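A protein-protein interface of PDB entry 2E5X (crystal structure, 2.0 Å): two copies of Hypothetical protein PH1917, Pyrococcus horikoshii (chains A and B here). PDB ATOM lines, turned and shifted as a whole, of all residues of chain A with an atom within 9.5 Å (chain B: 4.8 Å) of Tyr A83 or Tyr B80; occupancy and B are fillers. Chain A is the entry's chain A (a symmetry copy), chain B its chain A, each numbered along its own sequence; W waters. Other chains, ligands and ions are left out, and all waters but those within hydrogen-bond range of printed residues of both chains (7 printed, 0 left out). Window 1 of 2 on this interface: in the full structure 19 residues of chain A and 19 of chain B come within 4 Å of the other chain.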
ATOM      1  N   GLU A  36       7.747  10.211 -31.838  1.00  0.00           N
ATOM      2  CA  GLU A  36       8.959  10.403 -31.052  1.00  0.00           C
ATOM      3  C   GLU A  36       8.567  10.066 -29.621  1.00  0.00           C
ATOM      4  O   GLU A  36       7.748  10.755 -29.012  1.00  0.00           O
ATOM      5  CB  GLU A  36       9.447  11.850 -31.133  1.00  0.00           C
ATOM      6  CG  GLU A  36       9.776  12.322 -32.547  1.00  0.00           C
ATOM      7  CD  GLU A  36      10.234  13.765 -32.576  1.00  0.00           C
ATOM      8  OE1 GLU A  36       9.366  14.660 -32.487  1.00  0.00           O
ATOM      9  OE2 GLU A  36      11.456  14.005 -32.672  1.00  0.00           O
ATOM     10  N   ILE A  37       9.133   8.995 -29.085  1.00  0.00           N
ATOM     11  CA  ILE A  37       8.794   8.605 -27.731  1.00  0.00           C
ATOM     12  C   ILE A  37       9.532   9.437 -26.703  1.00  0.00           C
ATOM     13  O   ILE A  37      10.583  10.027 -26.986  1.00  0.00           O
ATOM     14  CB  ILE A  37       9.124   7.116 -27.458  1.00  0.00           C
ATOM     15  CG1 ILE A  37      10.602   6.848 -27.743  1.00  0.00           C
ATOM     16  CG2 ILE A  37       8.240   6.223 -28.304  1.00  0.00           C
ATOM     17  CD1 ILE A  37      11.064   5.456 -27.336  1.00  0.00           C
ATOM     18  N   GLN A  38       8.952   9.504 -25.515  1.00  0.00           N
ATOM     19  CA  GLN A  38       9.576  10.203 -24.412  1.00  0.00           C
ATOM     20  C   GLN A  38      10.595   9.182 -23.938  1.00  0.00           C
ATOM     21  O   GLN A  38      10.281   8.001 -23.797  1.00  0.00           O
ATOM     22  CB  GLN A  38       8.554  10.491 -23.306  1.00  0.00           C
ATOM     23  CG  GLN A  38       7.523  11.546 -23.689  1.00  0.00           C
ATOM     24  CD  GLN A  38       6.509  11.802 -22.588  1.00  0.00           C
ATOM     25  OE1 GLN A  38       6.876  11.985 -21.426  1.00  0.00           O
ATOM     26  NE2 GLN A  38       5.227  11.823 -22.949  1.00  0.00           N
ATOM     27  N   ALA A  39      11.819   9.622 -23.713  1.00  0.00           N
ATOM     28  CA  ALA A  39      12.857   8.709 -23.278  1.00  0.00           C
ATOM     29  C   ALA A  39      13.986   9.493 -22.652  1.00  0.00           C
ATOM     30  O   ALA A  39      14.022  10.724 -22.730  1.00  0.00           O
ATOM     31  CB  ALA A  39      13.373   7.906 -24.468  1.00  0.00           C
ATOM     32  N   ASP A  65      18.076  13.004 -33.944  1.00  0.00           N
ATOM     33  CA  ASP A  65      17.484  13.509 -32.725  1.00  0.00           C
ATOM     34  C   ASP A  65      18.645  14.037 -31.916  1.00  0.00           C
ATOM     35  O   ASP A  65      19.660  13.355 -31.743  1.00  0.00           O
ATOM     36  CB  ASP A  65      16.749  12.412 -31.960  1.00  0.00           C
ATOM     37  CG  ASP A  65      15.676  12.977 -31.052  1.00  0.00           C
ATOM     38  OD1 ASP A  65      14.950  13.886 -31.509  1.00  0.00           O
ATOM     39  OD2 ASP A  65      15.551  12.521 -29.896  1.00  0.00           O
ATOM     40  N   SER A  66      18.504  15.264 -31.441  1.00  0.00           N
ATOM     41  CA  SER A  66      19.566  15.896 -30.685  1.00  0.00           C
ATOM     42  C   SER A  66      19.015  16.809 -29.606  1.00  0.00           C
ATOM     43  O   SER A  66      17.827  17.140 -29.592  1.00  0.00           O
ATOM     44  CB  SER A  66      20.468  16.692 -31.639  1.00  0.00           C
ATOM     45  OG  SER A  66      19.689  17.474 -32.537  1.00  0.00           O
ATOM     46  N   GLY A  67      19.891  17.213 -28.695  1.00  0.00           N
ATOM     47  CA  GLY A  67      19.462  18.088 -27.631  1.00  0.00           C
ATOM     48  C   GLY A  67      20.613  18.741 -26.902  1.00  0.00           C
ATOM     49  O   GLY A  67      21.777  18.375 -27.072  1.00  0.00           O
ATOM     50  N   PHE A  76      18.515  19.084 -18.260  1.00  0.00           N
ATOM     51  CA  PHE A  76      17.421  19.770 -18.947  1.00  0.00           C
ATOM     52  C   PHE A  76      18.044  20.789 -19.917  1.00  0.00           C
ATOM     53  O   PHE A  76      19.115  21.334 -19.643  1.00  0.00           O
ATOM     54  CB  PHE A  76      16.537  20.445 -17.882  1.00  0.00           C
ATOM     55  CG  PHE A  76      15.585  21.485 -18.409  1.00  0.00           C
ATOM     56  CD1 PHE A  76      16.038  22.757 -18.759  1.00  0.00           C
ATOM     57  CD2 PHE A  76      14.215  21.220 -18.469  1.00  0.00           C
ATOM     58  CE1 PHE A  76      15.140  23.756 -19.154  1.00  0.00           C
ATOM     59  CE2 PHE A  76      13.312  22.206 -18.858  1.00  0.00           C
ATOM     60  CZ  PHE A  76      13.775  23.482 -19.202  1.00  0.00           C
ATOM     61  N   PRO A  77      17.402  21.036 -21.074  1.00  0.00           N
ATOM     62  CA  PRO A  77      16.146  20.465 -21.585  1.00  0.00           C
ATOM     63  C   PRO A  77      16.322  19.077 -22.210  1.00  0.00           C
ATOM     64  O   PRO A  77      15.357  18.326 -22.367  1.00  0.00           O
ATOM     65  CB  PRO A  77      15.689  21.507 -22.600  1.00  0.00           C
ATOM     66  CG  PRO A  77      16.990  21.988 -23.181  1.00  0.00           C
ATOM     67  CD  PRO A  77      17.884  22.118 -21.956  1.00  0.00           C
ATOM     68  N   GLY A  78      17.560  18.756 -22.582  1.00  0.00           N
ATOM     69  CA  GLY A  78      17.867  17.456 -23.159  1.00  0.00           C
ATOM     70  C   GLY A  78      17.004  16.966 -24.306  1.00  0.00           C
ATOM     71  O   GLY A  78      16.873  17.624 -25.339  1.00  0.00           O
ATOM     72  N   VAL A  79      16.417  15.787 -24.121  1.00  0.00           N
ATOM     73  CA  VAL A  79      15.574  15.169 -25.137  1.00  0.00           C
ATOM     74  C   VAL A  79      14.384  16.040 -25.537  1.00  0.00           C
ATOM     75  O   VAL A  79      13.831  15.877 -26.626  1.00  0.00           O
ATOM     76  CB  VAL A  79      15.066  13.783 -24.650  1.00  0.00           C
ATOM     77  CG1 VAL A  79      14.100  13.180 -25.669  1.00  0.00           C
ATOM     78  CG2 VAL A  79      16.256  12.850 -24.429  1.00  0.00           C
ATOM     79  N   TYR A  80      14.006  16.980 -24.676  1.00  0.00           N
ATOM     80  CA  TYR A  80      12.875  17.850 -24.973  1.00  0.00           C
ATOM     81  C   TYR A  80      13.325  19.259 -25.322  1.00  0.00           C
ATOM     82  O   TYR A  80      12.597  20.234 -25.102  1.00  0.00           O
ATOM     83  CB  TYR A  80      11.910  17.847 -23.785  1.00  0.00           C
ATOM     84  CG  TYR A  80      11.562  16.434 -23.370  1.00  0.00           C
ATOM     85  CD1 TYR A  80      10.921  15.569 -24.258  1.00  0.00           C
ATOM     86  CD2 TYR A  80      11.981  15.923 -22.142  1.00  0.00           C
ATOM     87  CE1 TYR A  80      10.716  14.224 -23.937  1.00  0.00           C
ATOM     88  CE2 TYR A  80      11.780  14.579 -21.809  1.00  0.00           C
ATOM     89  CZ  TYR A  80      11.152  13.736 -22.716  1.00  0.00           C
ATOM     90  OH  TYR A  80      10.987  12.400 -22.418  1.00  0.00           O
ATOM     91  N   SER A  81      14.526  19.355 -25.884  1.00  0.00           N
ATOM     92  CA  SER A  81      15.091  20.639 -26.286  1.00  0.00           C
ATOM     93  C   SER A  81      14.172  21.426 -27.217  1.00  0.00           C
ATOM     94  O   SER A  81      14.049  22.644 -27.086  1.00  0.00           O
ATOM     95  CB  SER A  81      16.449  20.436 -26.970  1.00  0.00           C
ATOM     96  OG  SER A  81      17.427  20.009 -26.037  1.00  0.00           O
ATOM     97  N   SER A  82      13.529  20.740 -28.157  1.00  0.00           N
ATOM     98  CA  SER A  82      12.636  21.424 -29.090  1.00  0.00           C
ATOM     99  C   SER A  82      11.434  22.057 -28.391  1.00  0.00           C
ATOM    100  O   SER A  82      11.150  23.244 -28.583  1.00  0.00           O
ATOM    101  CB  SER A  82      12.138  20.461 -30.168  1.00  0.00           C
ATOM    102  OG  SER A  82      11.212  21.124 -31.010  1.00  0.00           O
ATOM    103  N   TYR A  83      10.726  21.267 -27.587  1.00  0.00           N
ATOM    104  CA  TYR A  83       9.560  21.771 -26.872  1.00  0.00           C
ATOM    105  C   TYR A  83       9.919  22.968 -25.999  1.00  0.00           C
ATOM    106  O   TYR A  83       9.208  23.972 -25.987  1.00  0.00           O
ATOM    107  CB  TYR A  83       8.948  20.684 -25.988  1.00  0.00           C
ATOM    108  CG  TYR A  83       7.764  21.179 -25.176  1.00  0.00           C
ATOM    109  CD1 TYR A  83       6.548  21.488 -25.791  1.00  0.00           C
ATOM    110  CD2 TYR A  83       7.871  21.364 -23.796  1.00  0.00           C
ATOM    111  CE1 TYR A  83       5.465  21.971 -25.048  1.00  0.00           C
ATOM    112  CE2 TYR A  83       6.798  21.847 -23.045  1.00  0.00           C
ATOM    113  CZ  TYR A  83       5.600  22.148 -23.674  1.00  0.00           C
ATOM    114  OH  TYR A  83       4.544  22.624 -22.926  1.00  0.00           O
ATOM    115  N   VAL A  84      11.020  22.846 -25.264  1.00  0.00           N
ATOM    116  CA  VAL A  84      11.483  23.916 -24.380  1.00  0.00           C
ATOM    117  C   VAL A  84      11.824  25.174 -25.181  1.00  0.00           C
ATOM    118  O   VAL A  84      11.510  26.296 -24.771  1.00  0.00           O
ATOM    119  CB  VAL A  84      12.720  23.456 -23.562  1.00  0.00           C
ATOM    120  CG1 VAL A  84      13.272  24.612 -22.743  1.00  0.00           C
ATOM    121  CG2 VAL A  84      12.323  22.310 -22.620  1.00  0.00           C
ATOM    122  N   TYR A  85      12.456  24.986 -26.333  1.00  0.00           N
ATOM    123  CA  TYR A  85      12.817  26.116 -27.181  1.00  0.00           C
ATOM    124  C   TYR A  85      11.559  26.869 -27.625  1.00  0.00           C
ATOM    125  O   TYR A  85      11.536  28.099 -27.640  1.00  0.00           O
ATOM    126  CB  TYR A  85      13.586  25.633 -28.418  1.00  0.00           C
ATOM    127  CG  TYR A  85      13.923  26.744 -29.387  1.00  0.00           C
ATOM    128  CD1 TYR A  85      14.964  27.636 -29.122  1.00  0.00           C
ATOM    129  CD2 TYR A  85      13.169  26.935 -30.546  1.00  0.00           C
ATOM    130  CE1 TYR A  85      15.244  28.694 -29.984  1.00  0.00           C
ATOM    131  CE2 TYR A  85      13.440  27.991 -31.415  1.00  0.00           C
ATOM    132  CZ  TYR A  85      14.476  28.864 -31.126  1.00  0.00           C
ATOM    133  OH  TYR A  85      14.734  29.915 -31.970  1.00  0.00           O
ATOM    134  N   ARG A  86      10.511  26.124 -27.969  1.00  0.00           N
ATOM    135  CA  ARG A  86       9.259  26.717 -28.438  1.00  0.00           C
ATOM    136  C   ARG A  86       8.412  27.365 -27.347  1.00  0.00           C
ATOM    137  O   ARG A  86       7.534  28.186 -27.636  1.00  0.00           O
ATOM    138  CB  ARG A  86       8.414  25.657 -29.155  1.00  0.00           C
ATOM    139  CG  ARG A  86       8.985  25.198 -30.484  1.00  0.00           C
ATOM    140  CD  ARG A  86       8.053  24.210 -31.185  1.00  0.00           C
ATOM    141  NE  ARG A  86       8.064  22.880 -30.574  1.00  0.00           N
ATOM    142  CZ  ARG A  86       7.037  22.338 -29.927  1.00  0.00           C
ATOM    143  NH1 ARG A  86       5.899  23.006 -29.796  1.00  0.00           N
ATOM    144  NH2 ARG A  86       7.146  21.117 -29.421  1.00  0.00           N
ATOM    145  N   THR A  87       8.663  27.005 -26.096  1.00  0.00           N
ATOM    146  CA  THR A  87       7.882  27.566 -25.008  1.00  0.00           C
ATOM    147  C   THR A  87       8.599  28.658 -24.219  1.00  0.00           C
ATOM    148  O   THR A  87       8.241  29.832 -24.329  1.00  0.00           O
ATOM    149  CB  THR A  87       7.399  26.449 -24.056  1.00  0.00           C
ATOM    150  OG1 THR A  87       8.502  25.607 -23.698  1.00  0.00           O
ATOM    151  CG2 THR A  87       6.326  25.605 -24.745  1.00  0.00           C
ATOM    152  N   ILE A  88       9.604  28.298 -23.427  1.00  0.00           N
ATOM    153  CA  ILE A  88      10.307  29.314 -22.650  1.00  0.00           C
ATOM    154  C   ILE A  88      11.435  29.993 -23.431  1.00  0.00           C
ATOM    155  O   ILE A  88      11.909  31.054 -23.037  1.00  0.00           O
ATOM    156  CB  ILE A  88      10.863  28.738 -21.334  1.00  0.00           C
ATOM    157  CG1 ILE A  88      11.960  27.707 -21.618  1.00  0.00           C
ATOM    158  CG2 ILE A  88       9.727  28.112 -20.533  1.00  0.00           C
ATOM    159  CD1 ILE A  88      12.595  27.130 -20.356  1.00  0.00           C
ATOM    160  N   GLY A  89      11.857  29.379 -24.535  1.00  0.00           N
ATOM    161  CA  GLY A  89      12.905  29.955 -25.371  1.00  0.00           C
ATOM    162  C   GLY A  89      14.282  30.155 -24.755  1.00  0.00           C
ATOM    163  O   GLY A  89      14.563  29.680 -23.654  1.00  0.00           O
ATOM    164  N   LEU A  90      15.151  30.856 -25.481  1.00  0.00           N
ATOM    165  CA  LEU A  90      16.499  31.124 -25.002  1.00  0.00           C
ATOM    166  C   LEU A  90      16.439  31.997 -23.749  1.00  0.00           C
ATOM    167  O   LEU A  90      17.279  31.887 -22.854  1.00  0.00           O
ATOM    168  CB  LEU A  90      17.324  31.822 -26.090  1.00  0.00           C
ATOM    169  CG  LEU A  90      17.409  31.104 -27.443  1.00  0.00           C
ATOM    170  CD1 LEU A  90      18.307  31.899 -28.381  1.00  0.00           C
ATOM    171  CD2 LEU A  90      17.952  29.691 -27.253  1.00  0.00           C
ATOM    172  N   ILE A  93      16.041  29.800 -20.694  1.00  0.00           N
ATOM    173  CA  ILE A  93      17.293  29.163 -20.298  1.00  0.00           C
ATOM    174  C   ILE A  93      18.175  30.165 -19.555  1.00  0.00           C
ATOM    175  O   ILE A  93      18.709  29.859 -18.489  1.00  0.00           O
ATOM    176  CB  ILE A  93      18.067  28.635 -21.526  1.00  0.00           C
ATOM    177  CG1 ILE A  93      17.231  27.582 -22.259  1.00  0.00           C
ATOM    178  CG2 ILE A  93      19.411  28.058 -21.090  1.00  0.00           C
ATOM    179  CD1 ILE A  93      16.818  26.401 -21.400  1.00  0.00           C
ATOM    180  N   TYR A 142      19.354  26.886 -30.103  1.00  0.00           N
ATOM    181  CA  TYR A 142      20.213  27.343 -29.017  1.00  0.00           C
ATOM    182  C   TYR A 142      21.596  27.850 -29.441  1.00  0.00           C
ATOM    183  O   TYR A 142      22.408  28.204 -28.584  1.00  0.00           O
ATOM    184  CB  TYR A 142      20.398  26.208 -28.004  1.00  0.00           C
ATOM    185  CG  TYR A 142      19.113  25.714 -27.383  1.00  0.00           C
ATOM    186  CD1 TYR A 142      18.551  26.360 -26.286  1.00  0.00           C
ATOM    187  CD2 TYR A 142      18.448  24.606 -27.907  1.00  0.00           C
ATOM    188  CE1 TYR A 142      17.349  25.912 -25.721  1.00  0.00           C
ATOM    189  CE2 TYR A 142      17.251  24.152 -27.355  1.00  0.00           C
ATOM    190  CZ  TYR A 142      16.708  24.808 -26.264  1.00  0.00           C
ATOM    191  OH  TYR A 142      15.529  24.356 -25.720  1.00  0.00           O
ATOM    192  N   GLN B  38       5.831  11.562 -27.272  1.00  0.00           N
ATOM    193  CA  GLN B  38       5.923  13.000 -27.144  1.00  0.00           C
ATOM    194  C   GLN B  38       4.715  13.458 -27.943  1.00  0.00           C
ATOM    195  O   GLN B  38       4.470  12.970 -29.045  1.00  0.00           O
ATOM    196  CB  GLN B  38       7.215  13.519 -27.784  1.00  0.00           C
ATOM    197  CG  GLN B  38       8.473  13.141 -27.012  1.00  0.00           C
ATOM    198  CD  GLN B  38       9.743  13.648 -27.674  1.00  0.00           C
ATOM    199  OE1 GLN B  38       9.828  14.816 -28.058  1.00  0.00           O
ATOM    200  NE2 GLN B  38      10.738  12.773 -27.805  1.00  0.00           N
ATOM    201  N   ALA B  39       3.946  14.375 -27.385  1.00  0.00           N
ATOM    202  CA  ALA B  39       2.761  14.853 -28.072  1.00  0.00           C
ATOM    203  C   ALA B  39       2.339  16.178 -27.483  1.00  0.00           C
ATOM    204  O   ALA B  39       2.859  16.607 -26.449  1.00  0.00           O
ATOM    205  CB  ALA B  39       1.635  13.833 -27.932  1.00  0.00           C
ATOM    206  N   LYS B  74       3.851  29.769 -21.962  1.00  0.00           N
ATOM    207  CA  LYS B  74       3.272  29.199 -23.185  1.00  0.00           C
ATOM    208  C   LYS B  74       2.840  27.735 -23.038  1.00  0.00           C
ATOM    209  O   LYS B  74       2.946  26.944 -23.965  1.00  0.00           O
ATOM    210  CB  LYS B  74       4.288  29.318 -24.324  1.00  0.00           C
ATOM    211  CG  LYS B  74       4.496  30.763 -24.791  1.00  0.00           C
ATOM    212  CD  LYS B  74       5.526  30.851 -25.922  1.00  0.00           C
ATOM    213  CE  LYS B  74       5.577  32.229 -26.586  1.00  0.00           C
ATOM    214  NZ  LYS B  74       5.941  33.235 -25.588  1.00  0.00           N
ATOM    215  N   GLY B  75       2.328  27.368 -21.868  1.00  0.00           N
ATOM    216  CA  GLY B  75       1.871  26.005 -21.670  1.00  0.00           C
ATOM    217  C   GLY B  75       2.872  25.079 -21.011  1.00  0.00           C
ATOM    218  O   GLY B  75       2.502  24.003 -20.538  1.00  0.00           O
ATOM    219  N   PHE B  76       4.140  25.477 -20.996  1.00  0.00           N
ATOM    220  CA  PHE B  76       5.199  24.685 -20.370  1.00  0.00           C
ATOM    221  C   PHE B  76       4.885  24.592 -18.866  1.00  0.00           C
ATOM    222  O   PHE B  76       4.307  25.518 -18.293  1.00  0.00           O
ATOM    223  CB  PHE B  76       6.542  25.384 -20.644  1.00  0.00           C
ATOM    224  CG  PHE B  76       7.688  24.922 -19.785  1.00  0.00           C
ATOM    225  CD1 PHE B  76       7.802  25.344 -18.459  1.00  0.00           C
ATOM    226  CD2 PHE B  76       8.706  24.137 -20.329  1.00  0.00           C
ATOM    227  CE1 PHE B  76       8.919  24.996 -17.689  1.00  0.00           C
ATOM    228  CE2 PHE B  76       9.822  23.787 -19.573  1.00  0.00           C
ATOM    229  CZ  PHE B  76       9.932  24.219 -18.246  1.00  0.00           C
ATOM    230  N   PRO B  77       5.233  23.467 -18.215  1.00  0.00           N
ATOM    231  CA  PRO B  77       5.892  22.256 -18.730  1.00  0.00           C
ATOM    232  C   PRO B  77       4.932  21.305 -19.453  1.00  0.00           C
ATOM    233  O   PRO B  77       5.357  20.443 -20.225  1.00  0.00           O
ATOM    234  CB  PRO B  77       6.490  21.636 -17.473  1.00  0.00           C
ATOM    235  CG  PRO B  77       5.460  21.961 -16.427  1.00  0.00           C
ATOM    236  CD  PRO B  77       5.092  23.403 -16.746  1.00  0.00           C
ATOM    237  N   GLY B  78       3.639  21.459 -19.177  1.00  0.00           N
ATOM    238  CA  GLY B  78       2.622  20.641 -19.819  1.00  0.00           C
ATOM    239  C   GLY B  78       2.817  19.136 -19.822  1.00  0.00           C
ATOM    240  O   GLY B  78       2.957  18.505 -18.773  1.00  0.00           O
ATOM    241  N   VAL B  79       2.814  18.558 -21.019  1.00  0.00           N
ATOM    242  CA  VAL B  79       2.969  17.118 -21.188  1.00  0.00           C
ATOM    243  C   VAL B  79       4.270  16.582 -20.594  1.00  0.00           C
ATOM    244  O   VAL B  79       4.372  15.394 -20.284  1.00  0.00           O
ATOM    245  CB  VAL B  79       2.884  16.737 -22.692  1.00  0.00           C
ATOM    246  CG1 VAL B  79       3.148  15.244 -22.880  1.00  0.00           C
ATOM    247  CG2 VAL B  79       1.506  17.107 -23.238  1.00  0.00           C
ATOM    248  N   TYR B  80       5.256  17.456 -20.411  1.00  0.00           N
ATOM    249  CA  TYR B  80       6.535  17.029 -19.859  1.00  0.00           C
ATOM    250  C   TYR B  80       6.717  17.502 -18.427  1.00  0.00           C
ATOM    251  O   TYR B  80       7.841  17.715 -17.962  1.00  0.00           O
ATOM    252  CB  TYR B  80       7.666  17.528 -20.762  1.00  0.00           C
ATOM    253  CG  TYR B  80       7.415  17.153 -22.206  1.00  0.00           C
ATOM    254  CD1 TYR B  80       7.319  15.814 -22.587  1.00  0.00           C
ATOM    255  CD2 TYR B  80       7.153  18.130 -23.165  1.00  0.00           C
ATOM    256  CE1 TYR B  80       6.953  15.457 -23.888  1.00  0.00           C
ATOM    257  CE2 TYR B  80       6.788  17.784 -24.471  1.00  0.00           C
ATOM    258  CZ  TYR B  80       6.685  16.446 -24.821  1.00  0.00           C
ATOM    259  OH  TYR B  80       6.283  16.092 -26.092  1.00  0.00           O
ATOM    260  N   SER B  81       5.596  17.647 -17.725  1.00  0.00           N
ATOM    261  CA  SER B  81       5.608  18.084 -16.332  1.00  0.00           C
ATOM    262  C   SER B  81       6.500  17.218 -15.447  1.00  0.00           C
ATOM    263  O   SER B  81       7.204  17.735 -14.579  1.00  0.00           O
ATOM    264  CB  SER B  81       4.183  18.090 -15.761  1.00  0.00           C
ATOM    265  OG  SER B  81       3.408  19.124 -16.345  1.00  0.00           O
ATOM    266  N   SER B  82       6.473  15.906 -15.657  1.00  0.00           N
ATOM    267  CA  SER B  82       7.296  15.011 -14.846  1.00  0.00           C
ATOM    268  C   SER B  82       8.791  15.254 -15.040  1.00  0.00           C
ATOM    269  O   SER B  82       9.530  15.425 -14.066  1.00  0.00           O
ATOM    270  CB  SER B  82       6.982  13.548 -15.165  1.00  0.00           C
ATOM    271  OG  SER B  82       7.845  12.703 -14.428  1.00  0.00           O
ATOM    272  N   TYR B  83       9.237  15.262 -16.295  1.00  0.00           N
ATOM    273  CA  TYR B  83      10.647  15.486 -16.591  1.00  0.00           C
ATOM    274  C   TYR B  83      11.132  16.810 -16.011  1.00  0.00           C
ATOM    275  O   TYR B  83      12.203  16.877 -15.407  1.00  0.00           O
ATOM    276  CB  TYR B  83      10.896  15.488 -18.100  1.00  0.00           C
ATOM    277  CG  TYR B  83      12.342  15.777 -18.460  1.00  0.00           C
ATOM    278  CD1 TYR B  83      13.348  14.841 -18.206  1.00  0.00           C
ATOM    279  CD2 TYR B  83      12.707  17.000 -19.030  1.00  0.00           C
ATOM    280  CE1 TYR B  83      14.686  15.117 -18.512  1.00  0.00           C
ATOM    281  CE2 TYR B  83      14.039  17.286 -19.337  1.00  0.00           C
ATOM    282  CZ  TYR B  83      15.021  16.344 -19.078  1.00  0.00           C
ATOM    283  OH  TYR B  83      16.333  16.634 -19.384  1.00  0.00           O
ATOM    284  N   VAL B  84      10.343  17.860 -16.212  1.00  0.00           N
ATOM    285  CA  VAL B  84      10.685  19.191 -15.712  1.00  0.00           C
ATOM    286  C   VAL B  84      10.767  19.196 -14.185  1.00  0.00           C
ATOM    287  O   VAL B  84      11.662  19.809 -13.596  1.00  0.00           O
ATOM    288  CB  VAL B  84       9.645  20.242 -16.192  1.00  0.00           C
ATOM    289  CG1 VAL B  84       9.935  21.596 -15.565  1.00  0.00           C
ATOM    290  CG2 VAL B  84       9.700  20.366 -17.721  1.00  0.00           C
HETATM  291  O   HOH W   1       2.896  24.217 -24.339  1.00  0.00           O
HETATM  292  O   HOH W   2       5.488  12.037 -31.146  1.00  0.00           O
HETATM  293  O   HOH W   3       2.940  20.219 -23.409  1.00  0.00           O
HETATM  294  O   HOH W   4      13.160  13.963 -28.787  1.00  0.00           O
HETATM  295  O   HOH W   5      11.312  16.069 -29.993  1.00  0.00           O
HETATM  296  O   HOH W   6      16.443  14.578 -21.470  1.00  0.00           O
HETATM  297  O   HOH W   7       3.471  12.621 -20.822  1.00  0.00           O
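N of Ala B39 lies within hydrogen-bond range of OH of Tyr B80 (3.2 Å). OH of Tyr A80 is in hydrogen-bond range of N of Ala A39 (3.2 Å). O of Tyr A83 lies within hydrogen-bond range of OG1 of Thr A87. The side-chain hydroxyl (OG1) of Thr A87 sits at hydrogen-bond distance from the backbone carbonyl oxygen (O) of Val A84 (3.3 Å).
Tyr A83 touches just these residues of chain B: Gly B75 (3.4 Å), Phe B76 (3.3 Å), Pro B77 (3.5 Å) and Tyr B80 (3.4 Å). No residue of chain A comes within 4 Å of Gly B78. Of the printed residues of chain B, Phe A76 touches Phe B76 and Tyr B83. Printed residues of chain B within 4 Å of Ile A88: Phe B76 (3.9 Å). Of the printed residues of chain B, Tyr A80 touches Gln B38 (3.9 Å), Tyr B80 (3.96 Å) and Tyr B83 (3.4 Å). Printed residues of chain B within 4 Å of Thr A87: Lys B74 (3.3 Å) and Phe B76 (3.6 Å). The nearest residue of chain A that does not touch Tyr B80 is Arg A86 (6.0 Å).
The backbone NH of Gln B38 lies within hydrogen-bond range of the backbone carbonyl oxygen of Glu A36, at 2.7 Å. The backbone carbonyl oxygen (O) of Ile A37 lies within hydrogen-bond range of the side-chain amide nitrogen (NE2) of Gln B38 (2.9 Å). O of Gly B75 lies within hydrogen-bond range of OH of Tyr A83, at 3.4 Å. The backbone NH of Phe B76 sits close to the side-chain hydroxyl of Tyr A83, 3.5 Å away. The backbone NH of Phe A76 lies close to the side-chain hydroxyl of Tyr B83, at 3.5 Å.
Gln B38 touches its own counterpart, Gln A38. Phe A76 touches Tyr B83, and with the chains exchanged Tyr A83 touches Phe B76. Pro A77 touches Tyr B83, and with the chains exchanged Tyr A83 touches Pro B77. Tyr A80 touches Tyr B83, and with the chains exchanged Tyr A83 touches Tyr B80. Of the 18 pairs that touch across the chains among the printed residues, 11 have their exchanged pair printed and touching as well.
Printed residues of chain B that touch a printed residue of chain A: Gln B38, Lys B74, Gly B75, Phe B76, Pro B77, Tyr B80 and Tyr B83. Along chain B the printed residues that touch a printed residue of chain A span positions 38 to 83. Hydrophobic or aromatic side chains of chain A within 4 Å of the printed part of chain B: Phe A76, Tyr A80, Tyr A83 and Ile A88. Among the printed residues, no Asp or Glu carboxylate lies within 4 Å of a Lys or Arg side-chain nitrogen of the other chain.
Water W2 lies within hydrogen-bond range of O of Gln B38 and N of Glu A36. Water W1 bridges the side-chain hydroxyl of Tyr A83 and the backbone carbonyl oxygen of Lys B74. Water W5 lies within hydrogen-bond range of the side-chain amide oxygen of Gln B38 and the side-chain carboxylate of Glu A36. Water W7 lies within hydrogen-bond range of NE2 of Gln A38 (2.9 Å) and O of Val B79 (3.0 Å). Water W6 lies within hydrogen-bond range of N of Val A79 and OH of Tyr B83. Water W3 lies within hydrogen-bond range of N of Val B79 (2.9 Å) and OH of Tyr A83 (2.9 Å).
Among the printed residues, merely in contact across the chains: Thr A87 with Lys B74 (3.3 Å), Tyr A80 with Tyr B83 (3.4 Å), Tyr A83 with Tyr B80 (3.4 Å), Pro A77 with Tyr B83 (3.5 Å), Tyr A83 with Pro B77 (3.5 Å), Thr A87 with Phe B76 (3.6 Å), Arg A86 with Lys B74 (3.8 Å), Gln A38 with Gln B38 (3.8 Å), Ile A88 with Phe B76 (3.9 Å), Phe A76 with Phe B76 (3.9 Å), Tyr A80 with Gln B38 (3.9 Å), Gln A38 with Tyr B80 (3.9 Å) and Tyr A80 with Tyr B80 (3.96 Å).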
